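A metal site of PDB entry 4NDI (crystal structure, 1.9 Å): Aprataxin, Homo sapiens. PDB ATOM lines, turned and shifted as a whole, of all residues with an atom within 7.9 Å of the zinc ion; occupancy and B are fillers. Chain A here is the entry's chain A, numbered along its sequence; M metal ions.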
ATOM      1  N   ARG A 158     -11.809 -25.698 -31.533  1.00  0.00           N
ATOM      2  CA  ARG A 158     -11.391 -25.442 -30.176  1.00  0.00           C
ATOM      3  C   ARG A 158     -12.429 -25.992 -29.223  1.00  0.00           C
ATOM      4  O   ARG A 158     -13.625 -25.683 -29.347  1.00  0.00           O
ATOM      5  CB  ARG A 158     -11.233 -23.943 -29.940  1.00  0.00           C
ATOM      6  CG  ARG A 158     -10.693 -23.603 -28.557  1.00  0.00           C
ATOM      7  CD  ARG A 158     -10.802 -22.120 -28.215  1.00  0.00           C
ATOM      8  NE  ARG A 158     -10.029 -21.245 -29.102  1.00  0.00           N
ATOM      9  CZ  ARG A 158      -8.711 -21.073 -29.038  1.00  0.00           C
ATOM     10  NH1 ARG A 158      -7.996 -21.736 -28.133  1.00  0.00           N
ATOM     11  NH2 ARG A 158      -8.094 -20.242 -29.882  1.00  0.00           N
ATOM     12  N   CYS A 159     -11.988 -26.777 -28.243  1.00  0.00           N
ATOM     13  CA  CYS A 159     -12.883 -27.257 -27.184  1.00  0.00           C
ATOM     14  C   CYS A 159     -13.564 -26.109 -26.423  1.00  0.00           C
ATOM     15  O   CYS A 159     -12.918 -25.121 -26.042  1.00  0.00           O
ATOM     16  CB  CYS A 159     -12.142 -28.193 -26.226  1.00  0.00           C
ATOM     17  SG  CYS A 159     -13.214 -28.731 -24.896  1.00  0.00           S
ATOM     18  N   HIS A 160     -14.871 -26.230 -26.214  1.00  0.00           N
ATOM     19  CA  HIS A 160     -15.636 -25.199 -25.527  1.00  0.00           C
ATOM     20  C   HIS A 160     -15.470 -25.253 -24.005  1.00  0.00           C
ATOM     21  O   HIS A 160     -15.875 -24.327 -23.308  1.00  0.00           O
ATOM     22  CB  HIS A 160     -17.122 -25.342 -25.867  1.00  0.00           C
ATOM     23  CG  HIS A 160     -17.736 -26.627 -25.395  1.00  0.00           C
ATOM     24  ND1 HIS A 160     -17.145 -27.855 -25.627  1.00  0.00           N
ATOM     25  CD2 HIS A 160     -18.877 -26.879 -24.723  1.00  0.00           C
ATOM     26  CE1 HIS A 160     -17.900 -28.803 -25.093  1.00  0.00           C
ATOM     27  NE2 HIS A 160     -18.953 -28.240 -24.533  1.00  0.00           N
ATOM     28  N   GLU A 161     -14.902 -26.340 -23.484  1.00  0.00           N
ATOM     29  CA  GLU A 161     -14.741 -26.454 -22.024  1.00  0.00           C
ATOM     30  C   GLU A 161     -13.364 -25.997 -21.555  1.00  0.00           C
ATOM     31  O   GLU A 161     -13.255 -25.312 -20.532  1.00  0.00           O
ATOM     32  CB  GLU A 161     -15.023 -27.878 -21.531  1.00  0.00           C
ATOM     33  CG  GLU A 161     -16.451 -28.378 -21.776  1.00  0.00           C
ATOM     34  CD  GLU A 161     -17.501 -27.661 -20.930  1.00  0.00           C
ATOM     35  OE1 GLU A 161     -17.126 -26.906 -20.009  1.00  0.00           O
ATOM     36  OE2 GLU A 161     -18.711 -27.881 -21.186  1.00  0.00           O
ATOM     37  N   CYS A 162     -12.328 -26.352 -22.299  1.00  0.00           N
ATOM     38  CA  CYS A 162     -10.958 -26.107 -21.853  1.00  0.00           C
ATOM     39  C   CYS A 162     -10.123 -25.332 -22.872  1.00  0.00           C
ATOM     40  O   CYS A 162      -8.947 -25.093 -22.639  1.00  0.00           O
ATOM     41  CB  CYS A 162     -10.276 -27.433 -21.501  1.00  0.00           C
ATOM     42  SG  CYS A 162      -9.828 -28.463 -22.920  1.00  0.00           S
ATOM     43  N   GLN A 163     -10.730 -24.956 -24.002  1.00  0.00           N
ATOM     44  CA  GLN A 163     -10.061 -24.117 -24.995  1.00  0.00           C
ATOM     45  C   GLN A 163      -8.896 -24.805 -25.747  1.00  0.00           C
ATOM     46  O   GLN A 163      -8.193 -24.154 -26.538  1.00  0.00           O
ATOM     47  CB  GLN A 163      -9.584 -22.787 -24.383  1.00  0.00           C
ATOM     48  CG  GLN A 163     -10.699 -21.775 -24.071  1.00  0.00           C
ATOM     49  CD  GLN A 163     -11.692 -22.262 -23.025  1.00  0.00           C
ATOM     50  OE1 GLN A 163     -11.327 -22.490 -21.862  1.00  0.00           O
ATOM     51  NE2 GLN A 163     -12.952 -22.413 -23.420  1.00  0.00           N
ATOM     52  N   GLN A 164      -8.698 -26.095 -25.519  1.00  0.00           N
ATOM     53  CA  GLN A 164      -7.675 -26.827 -26.276  1.00  0.00           C
ATOM     54  C   GLN A 164      -8.020 -26.836 -27.758  1.00  0.00           C
ATOM     55  O   GLN A 164      -9.183 -26.969 -28.148  1.00  0.00           O
ATOM     56  CB  GLN A 164      -7.513 -28.257 -25.779  1.00  0.00           C
ATOM     57  CG  GLN A 164      -6.394 -29.029 -26.491  1.00  0.00           C
ATOM     58  CD  GLN A 164      -6.049 -30.350 -25.818  1.00  0.00           C
ATOM     59  OE1 GLN A 164      -6.142 -30.473 -24.591  1.00  0.00           O
ATOM     60  NE2 GLN A 164      -5.674 -31.355 -26.617  1.00  0.00           N
ATOM     61  N   LEU A 165      -6.999 -26.690 -28.600  1.00  0.00           N
ATOM     62  CA  LEU A 165      -7.167 -26.741 -30.050  1.00  0.00           C
ATOM     63  C   LEU A 165      -7.017 -28.183 -30.531  1.00  0.00           C
ATOM     64  O   LEU A 165      -6.080 -28.875 -30.136  1.00  0.00           O
ATOM     65  CB  LEU A 165      -6.127 -25.823 -30.719  1.00  0.00           C
ATOM     66  CG  LEU A 165      -6.355 -24.337 -30.438  1.00  0.00           C
ATOM     67  CD1 LEU A 165      -5.126 -23.475 -30.745  1.00  0.00           C
ATOM     68  CD2 LEU A 165      -7.595 -23.806 -31.188  1.00  0.00           C
ATOM     69  N   LEU A 166      -7.948 -28.619 -31.380  1.00  0.00           N
ATOM     70  CA  LEU A 166      -7.960 -29.988 -31.921  1.00  0.00           C
ATOM     71  C   LEU A 166      -7.843 -29.943 -33.435  1.00  0.00           C
ATOM     72  O   LEU A 166      -8.399 -29.062 -34.069  1.00  0.00           O
ATOM     73  CB  LEU A 166      -9.260 -30.712 -31.516  1.00  0.00           C
ATOM     74  CG  LEU A 166      -9.376 -31.288 -30.087  1.00  0.00           C
ATOM     75  CD1 LEU A 166      -8.134 -32.131 -29.676  1.00  0.00           C
ATOM     76  CD2 LEU A 166      -9.645 -30.204 -29.069  1.00  0.00           C
ATOM     77  N   LEU A 172     -11.566 -34.219 -32.002  1.00  0.00           N
ATOM     78  CA  LEU A 172     -12.397 -33.377 -31.141  1.00  0.00           C
ATOM     79  C   LEU A 172     -13.422 -34.236 -30.401  1.00  0.00           C
ATOM     80  O   LEU A 172     -13.631 -34.077 -29.203  1.00  0.00           O
ATOM     81  CB  LEU A 172     -13.117 -32.288 -31.939  1.00  0.00           C
ATOM     82  CG  LEU A 172     -14.089 -31.419 -31.131  1.00  0.00           C
ATOM     83  CD1 LEU A 172     -13.356 -30.668 -30.006  1.00  0.00           C
ATOM     84  CD2 LEU A 172     -14.813 -30.434 -32.054  1.00  0.00           C
ATOM     85  N   HIS A 175     -11.753 -36.105 -27.664  1.00  0.00           N
ATOM     86  CA  HIS A 175     -11.398 -35.180 -26.585  1.00  0.00           C
ATOM     87  C   HIS A 175     -12.589 -34.815 -25.692  1.00  0.00           C
ATOM     88  O   HIS A 175     -12.450 -34.727 -24.476  1.00  0.00           O
ATOM     89  CB  HIS A 175     -10.770 -33.894 -27.156  1.00  0.00           C
ATOM     90  CG  HIS A 175     -10.552 -32.820 -26.138  1.00  0.00           C
ATOM     91  ND1 HIS A 175      -9.396 -32.737 -25.384  1.00  0.00           N
ATOM     92  CD2 HIS A 175     -11.336 -31.797 -25.736  1.00  0.00           C
ATOM     93  CE1 HIS A 175      -9.489 -31.699 -24.565  1.00  0.00           C
ATOM     94  NE2 HIS A 175     -10.655 -31.114 -24.761  1.00  0.00           N
ATOM     95  N   LEU A 176     -13.754 -34.590 -26.311  1.00  0.00           N
ATOM     96  CA  LEU A 176     -14.940 -34.128 -25.591  1.00  0.00           C
ATOM     97  C   LEU A 176     -15.390 -35.137 -24.526  1.00  0.00           C
ATOM     98  O   LEU A 176     -16.006 -34.736 -23.538  1.00  0.00           O
ATOM     99  CB  LEU A 176     -16.103 -33.840 -26.554  1.00  0.00           C
ATOM    100  CG  LEU A 176     -15.992 -32.652 -27.506  1.00  0.00           C
ATOM    101  CD1 LEU A 176     -17.069 -32.738 -28.598  1.00  0.00           C
ATOM    102  CD2 LEU A 176     -16.075 -31.327 -26.757  1.00  0.00           C
ATOM    103  N   ARG A 177     -15.064 -36.414 -24.736  1.00  0.00           N
ATOM    104  CA  ARG A 177     -15.332 -37.474 -23.753  1.00  0.00           C
ATOM    105  C   ARG A 177     -14.855 -37.119 -22.362  1.00  0.00           C
ATOM    106  O   ARG A 177     -15.508 -37.445 -21.359  1.00  0.00           O
ATOM    107  CB  ARG A 177     -14.654 -38.793 -24.162  1.00  0.00           C
ATOM    108  CG  ARG A 177     -15.270 -39.502 -25.361  1.00  0.00           C
ATOM    109  CD  ARG A 177     -14.511 -40.790 -25.662  1.00  0.00           C
ATOM    110  NE  ARG A 177     -14.396 -41.647 -24.484  1.00  0.00           N
ATOM    111  CZ  ARG A 177     -13.423 -42.519 -24.285  1.00  0.00           C
ATOM    112  NH1 ARG A 177     -13.396 -43.255 -23.185  1.00  0.00           N
ATOM    113  NH2 ARG A 177     -12.466 -42.662 -25.199  1.00  0.00           N
ATOM    114  N   LYS A 178     -13.690 -36.471 -22.284  1.00  0.00           N
ATOM    115  CA  LYS A 178     -13.134 -36.149 -20.976  1.00  0.00           C
ATOM    116  C   LYS A 178     -14.008 -35.149 -20.200  1.00  0.00           C
ATOM    117  O   LYS A 178     -13.837 -35.010 -18.995  1.00  0.00           O
ATOM    118  CB  LYS A 178     -11.704 -35.623 -21.116  1.00  0.00           C
ATOM    119  CG  LYS A 178     -11.617 -34.156 -21.514  1.00  0.00           C
ATOM    120  CD  LYS A 178     -10.416 -33.474 -20.888  1.00  0.00           C
ATOM    121  CE  LYS A 178      -9.108 -34.043 -21.387  1.00  0.00           C
ATOM    122  NZ  LYS A 178      -7.957 -33.402 -20.696  1.00  0.00           N
ATOM    123  N   HIS A 179     -14.922 -34.470 -20.886  1.00  0.00           N
ATOM    124  CA  HIS A 179     -15.762 -33.469 -20.220  1.00  0.00           C
ATOM    125  C   HIS A 179     -17.184 -33.951 -19.878  1.00  0.00           C
ATOM    126  O   HIS A 179     -18.032 -33.156 -19.474  1.00  0.00           O
ATOM    127  CB  HIS A 179     -15.848 -32.196 -21.067  1.00  0.00           C
ATOM    128  CG  HIS A 179     -14.516 -31.578 -21.364  1.00  0.00           C
ATOM    129  ND1 HIS A 179     -13.655 -31.152 -20.370  1.00  0.00           N
ATOM    130  CD2 HIS A 179     -13.898 -31.325 -22.536  1.00  0.00           C
ATOM    131  CE1 HIS A 179     -12.559 -30.655 -20.924  1.00  0.00           C
ATOM    132  NE2 HIS A 179     -12.679 -30.750 -22.238  1.00  0.00           N
HETATM  133 ZN    ZN M   1     -11.576 -29.721 -23.589  1.00  0.00          ZN
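The zinc ion is bound by NE2 of His 179 (2.0 Å), NE2 of His 175 (2.0 Å), SG of Cys 162 (2.3 Å) and SG of Cys 159 (2.3 Å).
The backbone NH of Gln 164 lies close to the side-chain sulfur of Cys 162 (3.7 Å).
The side-chain sulfur of Cys 159 sits close to the backbone NH of Glu 161 (3.2 Å).
The backbone NH of Cys 159 sits at hydrogen-bond distance from the backbone carbonyl oxygen of Gln 164, at 2.8 Å.
Within 4 Å of the zinc ion: Cys 159, Cys 162, His 175 and His 179.
Along chain A the residues within 4 Å of the zinc ion span positions 159 to 179.
The nearest printed residue that does not touch the zinc ion is Glu 161 (4.4 Å).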
